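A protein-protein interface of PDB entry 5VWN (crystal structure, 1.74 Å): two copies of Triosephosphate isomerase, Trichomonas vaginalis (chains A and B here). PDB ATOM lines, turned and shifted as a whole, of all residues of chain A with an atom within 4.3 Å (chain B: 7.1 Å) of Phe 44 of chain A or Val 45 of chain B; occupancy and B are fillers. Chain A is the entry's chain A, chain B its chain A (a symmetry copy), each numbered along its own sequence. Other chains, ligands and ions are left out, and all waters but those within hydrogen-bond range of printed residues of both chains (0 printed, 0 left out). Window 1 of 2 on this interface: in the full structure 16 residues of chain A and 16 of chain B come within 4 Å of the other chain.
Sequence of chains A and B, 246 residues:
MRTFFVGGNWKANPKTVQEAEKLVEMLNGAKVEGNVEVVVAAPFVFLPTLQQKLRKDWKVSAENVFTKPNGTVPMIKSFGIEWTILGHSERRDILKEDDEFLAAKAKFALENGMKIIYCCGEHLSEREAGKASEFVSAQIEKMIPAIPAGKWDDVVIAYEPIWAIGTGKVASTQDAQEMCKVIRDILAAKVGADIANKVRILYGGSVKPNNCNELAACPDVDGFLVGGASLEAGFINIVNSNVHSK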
ATOM      1  N   ALA A  42     -16.339 -35.131  14.043  1.00  0.00           N
ATOM      2  CA  ALA A  42     -15.972 -34.724  12.689  1.00  0.00           C
ATOM      3  C   ALA A  42     -14.473 -34.887  12.475  1.00  0.00           C
ATOM      4  O   ALA A  42     -13.718 -35.023  13.438  1.00  0.00           O
ATOM      5  CB  ALA A  42     -16.364 -33.260  12.434  1.00  0.00           C
ATOM      6  N   PRO A  43     -14.011 -34.880  11.215  1.00  0.00           N
ATOM      7  CA  PRO A  43     -12.560 -34.913  10.966  1.00  0.00           C
ATOM      8  C   PRO A  43     -11.835 -33.779  11.686  1.00  0.00           C
ATOM      9  O   PRO A  43     -12.399 -32.707  11.911  1.00  0.00           O
ATOM     10  CB  PRO A  43     -12.462 -34.753   9.438  1.00  0.00           C
ATOM     11  CG  PRO A  43     -13.755 -35.336   8.921  1.00  0.00           C
ATOM     12  CD  PRO A  43     -14.800 -34.994   9.972  1.00  0.00           C
ATOM     13  N   PHE A  44     -10.554 -34.017  12.021  1.00  0.00           N
ATOM     14  CA  PHE A  44      -9.790 -33.048  12.807  1.00  0.00           C
ATOM     15  C   PHE A  44      -9.789 -31.662  12.173  1.00  0.00           C
ATOM     16  O   PHE A  44      -9.925 -30.660  12.880  1.00  0.00           O
ATOM     17  CB  PHE A  44      -8.338 -33.515  13.010  1.00  0.00           C
ATOM     18  CG  PHE A  44      -8.192 -34.684  13.941  1.00  0.00           C
ATOM     19  CD1 PHE A  44      -8.344 -34.517  15.313  1.00  0.00           C
ATOM     20  CD2 PHE A  44      -7.906 -35.947  13.446  1.00  0.00           C
ATOM     21  CE1 PHE A  44      -8.220 -35.611  16.171  1.00  0.00           C
ATOM     22  CE2 PHE A  44      -7.774 -37.021  14.289  1.00  0.00           C
ATOM     23  CZ  PHE A  44      -7.936 -36.857  15.648  1.00  0.00           C
ATOM     24  N   VAL A  45      -9.599 -31.574  10.846  1.00  0.00           N
ATOM     25  CA  VAL A  45      -9.484 -30.250  10.229  1.00  0.00           C
ATOM     26  C   VAL A  45     -10.791 -29.479  10.256  1.00  0.00           C
ATOM     27  O   VAL A  45     -10.778 -28.255  10.094  1.00  0.00           O
ATOM     28  CB  VAL A  45      -8.955 -30.338   8.778  1.00  0.00           C
ATOM     29  CG1 VAL A  45      -7.546 -30.882   8.780  1.00  0.00           C
ATOM     30  CG2 VAL A  45      -9.884 -31.186   7.885  1.00  0.00           C
ATOM     31  N   PHE A  46     -11.926 -30.158  10.484  1.00  0.00           N
ATOM     32  CA  PHE A  46     -13.210 -29.483  10.627  1.00  0.00           C
ATOM     33  C   PHE A  46     -13.591 -29.174  12.073  1.00  0.00           C
ATOM     34  O   PHE A  46     -14.585 -28.468  12.289  1.00  0.00           O
ATOM     35  CB  PHE A  46     -14.331 -30.331  10.001  1.00  0.00           C
ATOM     36  CG  PHE A  46     -14.168 -30.569   8.530  1.00  0.00           C
ATOM     37  CD1 PHE A  46     -13.415 -29.702   7.743  1.00  0.00           C
ATOM     38  CD2 PHE A  46     -14.782 -31.664   7.926  1.00  0.00           C
ATOM     39  CE1 PHE A  46     -13.271 -29.921   6.357  1.00  0.00           C
ATOM     40  CE2 PHE A  46     -14.644 -31.893   6.568  1.00  0.00           C
ATOM     41  CZ  PHE A  46     -13.879 -31.029   5.782  1.00  0.00           C
ATOM     42  N   LEU A  47     -12.861 -29.688  13.069  1.00  0.00           N
ATOM     43  CA  LEU A  47     -13.256 -29.424  14.454  1.00  0.00           C
ATOM     44  C   LEU A  47     -13.306 -27.936  14.809  1.00  0.00           C
ATOM     45  O   LEU A  47     -14.245 -27.539  15.524  1.00  0.00           O
ATOM     46  CB  LEU A  47     -12.343 -30.201  15.413  1.00  0.00           C
ATOM     47  CG  LEU A  47     -12.494 -31.726  15.336  1.00  0.00           C
ATOM     48  CD1 LEU A  47     -11.489 -32.465  16.233  1.00  0.00           C
ATOM     49  CD2 LEU A  47     -13.919 -32.197  15.658  1.00  0.00           C
ATOM     50  N   PRO A  48     -12.375 -27.068  14.367  1.00  0.00           N
ATOM     51  CA  PRO A  48     -12.527 -25.639  14.697  1.00  0.00           C
ATOM     52  C   PRO A  48     -13.803 -25.022  14.130  1.00  0.00           C
ATOM     53  O   PRO A  48     -14.478 -24.246  14.825  1.00  0.00           O
ATOM     54  CB  PRO A  48     -11.254 -25.004  14.095  1.00  0.00           C
ATOM     55  CG  PRO A  48     -10.239 -26.120  14.111  1.00  0.00           C
ATOM     56  CD  PRO A  48     -11.077 -27.327  13.695  1.00  0.00           C
ATOM     57  N   ASN A  64     -10.984 -39.479  17.582  1.00  0.00           N
ATOM     58  CA  ASN A  64      -9.958 -40.305  18.218  1.00  0.00           C
ATOM     59  C   ASN A  64      -9.002 -39.346  18.917  1.00  0.00           C
ATOM     60  O   ASN A  64      -9.026 -38.140  18.667  1.00  0.00           O
ATOM     61  CB  ASN A  64      -9.223 -41.178  17.192  1.00  0.00           C
ATOM     62  CG  ASN A  64      -8.415 -42.296  17.829  1.00  0.00           C
ATOM     63  OD1 ASN A  64      -8.502 -42.551  19.035  1.00  0.00           O
ATOM     64  ND2 ASN A  64      -7.629 -42.984  17.008  1.00  0.00           N
ATOM     65  N   MET A  75      -4.512 -30.333  22.643  1.00  0.00           N
ATOM     66  CA  MET A  75      -4.826 -29.554  21.445  1.00  0.00           C
ATOM     67  C   MET A  75      -6.327 -29.371  21.286  1.00  0.00           C
ATOM     68  O   MET A  75      -6.804 -28.257  21.052  1.00  0.00           O
ATOM     69  CB  MET A  75      -4.251 -30.232  20.195  1.00  0.00           C
ATOM     70  CG  MET A  75      -2.757 -30.429  20.194  1.00  0.00           C
ATOM     71  SD  MET A  75      -2.314 -31.155  18.592  1.00  0.00           S
ATOM     72  CE  MET A  75      -0.568 -31.458  18.865  1.00  0.00           C
ATOM     73  N   PHE A  79      -9.507 -25.774  22.194  1.00  0.00           N
ATOM     74  CA  PHE A  79     -10.645 -25.223  21.479  1.00  0.00           C
ATOM     75  C   PHE A  79     -11.934 -25.270  22.286  1.00  0.00           C
ATOM     76  O   PHE A  79     -12.947 -24.738  21.822  1.00  0.00           O
ATOM     77  CB  PHE A  79     -10.886 -25.989  20.178  1.00  0.00           C
ATOM     78  CG  PHE A  79      -9.836 -25.761  19.135  1.00  0.00           C
ATOM     79  CD1 PHE A  79      -9.928 -24.684  18.270  1.00  0.00           C
ATOM     80  CD2 PHE A  79      -8.773 -26.639  19.004  1.00  0.00           C
ATOM     81  CE1 PHE A  79      -8.959 -24.483  17.287  1.00  0.00           C
ATOM     82  CE2 PHE A  79      -7.813 -26.439  18.037  1.00  0.00           C
ATOM     83  CZ  PHE A  79      -7.904 -25.368  17.186  1.00  0.00           C
ATOM     84  N   VAL B  17      -3.895 -24.208  20.724  1.00  0.00           N
ATOM     85  CA  VAL B  17      -4.091 -23.297  19.595  1.00  0.00           C
ATOM     86  C   VAL B  17      -3.633 -21.892  19.954  1.00  0.00           C
ATOM     87  O   VAL B  17      -3.180 -21.141  19.083  1.00  0.00           O
ATOM     88  CB  VAL B  17      -5.559 -23.306  19.116  1.00  0.00           C
ATOM     89  CG1 VAL B  17      -6.481 -22.648  20.147  1.00  0.00           C
ATOM     90  CG2 VAL B  17      -5.695 -22.603  17.737  1.00  0.00           C
ATOM     91  N   ALA B  42       1.891 -28.424  10.249  1.00  0.00           N
ATOM     92  CA  ALA B  42       1.347 -28.348  11.603  1.00  0.00           C
ATOM     93  C   ALA B  42       0.311 -29.443  11.819  1.00  0.00           C
ATOM     94  O   ALA B  42      -0.174 -30.040  10.857  1.00  0.00           O
ATOM     95  CB  ALA B  42       0.696 -26.978  11.852  1.00  0.00           C
ATOM     96  N   PRO B  43      -0.047 -29.733  13.080  1.00  0.00           N
ATOM     97  CA  PRO B  43      -1.130 -30.699  13.331  1.00  0.00           C
ATOM     98  C   PRO B  43      -2.417 -30.309  12.607  1.00  0.00           C
ATOM     99  O   PRO B  43      -2.682 -29.127  12.378  1.00  0.00           O
ATOM    100  CB  PRO B  43      -1.310 -30.634  14.858  1.00  0.00           C
ATOM    101  CG  PRO B  43       0.051 -30.238  15.375  1.00  0.00           C
ATOM    102  CD  PRO B  43       0.627 -29.304  14.322  1.00  0.00           C
ATOM    103  N   PHE B  44      -3.236 -31.321  12.275  1.00  0.00           N
ATOM    104  CA  PHE B  44      -4.445 -31.083  11.486  1.00  0.00           C
ATOM    105  C   PHE B  44      -5.346 -30.026  12.115  1.00  0.00           C
ATOM    106  O   PHE B  44      -5.892 -29.177  11.405  1.00  0.00           O
ATOM    107  CB  PHE B  44      -5.248 -32.380  11.288  1.00  0.00           C
ATOM    108  CG  PHE B  44      -4.600 -33.368  10.360  1.00  0.00           C
ATOM    109  CD1 PHE B  44      -4.589 -33.148   8.988  1.00  0.00           C
ATOM    110  CD2 PHE B  44      -3.999 -34.513  10.861  1.00  0.00           C
ATOM    111  CE1 PHE B  44      -3.973 -34.064   8.134  1.00  0.00           C
ATOM    112  CE2 PHE B  44      -3.401 -35.420  10.022  1.00  0.00           C
ATOM    113  CZ  PHE B  44      -3.382 -35.194   8.662  1.00  0.00           C
ATOM    114  N   VAL B  45      -5.549 -30.078  13.442  1.00  0.00           N
ATOM    115  CA  VAL B  45      -6.497 -29.142  14.055  1.00  0.00           C
ATOM    116  C   VAL B  45      -6.002 -27.708  14.023  1.00  0.00           C
ATOM    117  O   VAL B  45      -6.806 -26.783  14.181  1.00  0.00           O
ATOM    118  CB  VAL B  45      -6.844 -29.546  15.507  1.00  0.00           C
ATOM    119  CG1 VAL B  45      -7.564 -30.875  15.509  1.00  0.00           C
ATOM    120  CG2 VAL B  45      -5.588 -29.586  16.402  1.00  0.00           C
ATOM    121  N   PHE B  46      -4.698 -27.489  13.796  1.00  0.00           N
ATOM    122  CA  PHE B  46      -4.158 -26.143  13.649  1.00  0.00           C
ATOM    123  C   PHE B  46      -4.067 -25.666  12.201  1.00  0.00           C
ATOM    124  O   PHE B  46      -3.767 -24.485  11.981  1.00  0.00           O
ATOM    125  CB  PHE B  46      -2.756 -26.059  14.276  1.00  0.00           C
ATOM    126  CG  PHE B  46      -2.727 -26.340  15.749  1.00  0.00           C
ATOM    127  CD1 PHE B  46      -3.863 -26.166  16.533  1.00  0.00           C
ATOM    128  CD2 PHE B  46      -1.550 -26.773  16.356  1.00  0.00           C
ATOM    129  CE1 PHE B  46      -3.833 -26.421  17.920  1.00  0.00           C
ATOM    130  CE2 PHE B  46      -1.508 -27.032  17.714  1.00  0.00           C
ATOM    131  CZ  PHE B  46      -2.652 -26.868  18.499  1.00  0.00           C
ATOM    132  N   LEU B  47      -4.287 -26.534  11.208  1.00  0.00           N
ATOM    133  CA  LEU B  47      -4.156 -26.082   9.821  1.00  0.00           C
ATOM    134  C   LEU B  47      -5.083 -24.918   9.462  1.00  0.00           C
ATOM    135  O   LEU B  47      -4.624 -24.010   8.744  1.00  0.00           O
ATOM    136  CB  LEU B  47      -4.345 -27.269   8.867  1.00  0.00           C
ATOM    137  CG  LEU B  47      -3.241 -28.332   8.949  1.00  0.00           C
ATOM    138  CD1 LEU B  47      -3.526 -29.549   8.056  1.00  0.00           C
ATOM    139  CD2 LEU B  47      -1.851 -27.767   8.626  1.00  0.00           C
ATOM    140  N   PRO B  48      -6.355 -24.860   9.901  1.00  0.00           N
ATOM    141  CA  PRO B  48      -7.166 -23.675   9.566  1.00  0.00           C
ATOM    142  C   PRO B  48      -6.595 -22.376  10.129  1.00  0.00           C
ATOM    143  O   PRO B  48      -6.584 -21.350   9.430  1.00  0.00           O
ATOM    144  CB  PRO B  48      -8.546 -24.015  10.167  1.00  0.00           C
ATOM    145  CG  PRO B  48      -8.596 -25.523  10.157  1.00  0.00           C
ATOM    146  CD  PRO B  48      -7.176 -25.897  10.576  1.00  0.00           C
ATOM    147  N   THR B  49      -6.132 -22.399  11.383  1.00  0.00           N
ATOM    148  CA  THR B  49      -5.491 -21.233  11.983  1.00  0.00           C
ATOM    149  C   THR B  49      -4.324 -20.745  11.135  1.00  0.00           C
ATOM    150  O   THR B  49      -4.212 -19.551  10.842  1.00  0.00           O
ATOM    151  CB  THR B  49      -5.002 -21.574  13.393  1.00  0.00           C
ATOM    152  OG1 THR B  49      -6.119 -21.965  14.198  1.00  0.00           O
ATOM    153  CG2 THR B  49      -4.325 -20.376  14.022  1.00  0.00           C
ATOM    154  N   LEU B  50      -3.427 -21.656  10.756  1.00  0.00           N
ATOM    155  CA  LEU B  50      -2.244 -21.252   9.999  1.00  0.00           C
ATOM    156  C   LEU B  50      -2.628 -20.726   8.629  1.00  0.00           C
ATOM    157  O   LEU B  50      -2.116 -19.691   8.185  1.00  0.00           O
ATOM    158  CB  LEU B  50      -1.268 -22.427   9.878  1.00  0.00           C
ATOM    159  CG  LEU B  50      -0.153 -22.474  10.917  1.00  0.00           C
ATOM    160  CD1 LEU B  50      -0.715 -22.705  12.344  1.00  0.00           C
ATOM    161  CD2 LEU B  50       0.860 -23.555  10.555  1.00  0.00           C
ATOM    162  N   MET B  75     -10.211 -32.475   1.648  1.00  0.00           N
ATOM    163  CA  MET B  75     -10.479 -31.674   2.843  1.00  0.00           C
ATOM    164  C   MET B  75      -9.455 -30.561   2.998  1.00  0.00           C
ATOM    165  O   MET B  75      -9.815 -29.403   3.228  1.00  0.00           O
ATOM    166  CB  MET B  75     -10.477 -32.559   4.096  1.00  0.00           C
ATOM    167  CG  MET B  75     -11.487 -33.678   4.100  1.00  0.00           C
ATOM    168  SD  MET B  75     -11.356 -34.511   5.704  1.00  0.00           S
ATOM    169  CE  MET B  75     -12.488 -35.875   5.435  1.00  0.00           C
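Phe 44 of chain A touches its own counterpart, Phe 44 of chain B.
Phe 44 of chain A touches Val 45 of chain B, and with the chains exchanged Val 45 of chain A touches Phe 44 of chain B.
Val 45 of chain A touches Pro 48 of chain B, and with the chains exchanged Pro 48 of chain A touches Val 45 of chain B.
Phe 46 of chain A touches Met 75 of chain B, and with the chains exchanged Met 75 of chain A touches Phe 46 of chain B.
8 positions are printed for both chains.
Of the 12 pairs that touch across the chains among the printed residues, 9 have their exchanged pair printed and touching as well.
Printed residues of chain B that touch a printed residue of chain A: Val 17, Pro 43, Phe 44, Val 45, Phe 46, Pro 48 and Met 75.
Hydrophobic or aromatic side chains of chain B that line the printed part of chain A: Val 17, Pro 43, Phe 44, Val 45, Phe 46, Pro 48 and Met 75.
Of the 10 printed residues of chain A, 7 touch a printed residue of chain B.
Hydrophobic or aromatic side chains of chain A that line the printed part of chain B: Pro 43, Phe 44, Val 45, Phe 46, Pro 48, Met 75 and Phe 79.
Among the printed residues, 12 pairs touch across the chains.
Among the printed residues, no Asp or Glu carboxylate lies within 4 Å of a Lys or Arg side-chain nitrogen of the other chain.
Phe 44 of chain A touches two residues of chain B.
Val 45 of chain B touches three residues of chain A.
Of the printed residues of chain B, Phe 46 of chain A touches Met 75.
Of the printed residues of chain B, Val 45 of chain A touches Phe 44 (3.5 Å) and Pro 48 (3.5 Å).
Of the printed residues of chain B, Pro 43 of chain A touches Met 75 (3.7 Å).
Of the printed residues of chain A, Pro 43 of chain B touches Met 75.
The nearest printed residue of chain B that does not touch Phe 46 of chain A is Pro 48 of chain B (5.7 Å).
CG of Pro 43 of chain A touches CE of Met 75 of chain B, 3.7 Å away.
Phe 44 of chain A touches Phe 44 of chain B.
O of Phe 44 of chain A touches CG1 of Val 45 of chain B, 3.5 Å away.
O of Phe 44 of chain B touches CG1 of Val 45 of chain A, at 3.5 Å.
CG of Pro 48 of chain B touches O of Val 45 of chain A, at 3.5 Å.
Phe 46 of chain A touches Met 75 of chain B.
CG of Pro 48 of chain A touches O of Val 45 of chain B (3.5 Å).
Met 75 of chain A touches Pro 43 of chain B.
Phe 46 of chain B touches Met 75 of chain A (CZ to CG, 3.9 Å).
Phe 79 of chain A touches Val 45 of chain B.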
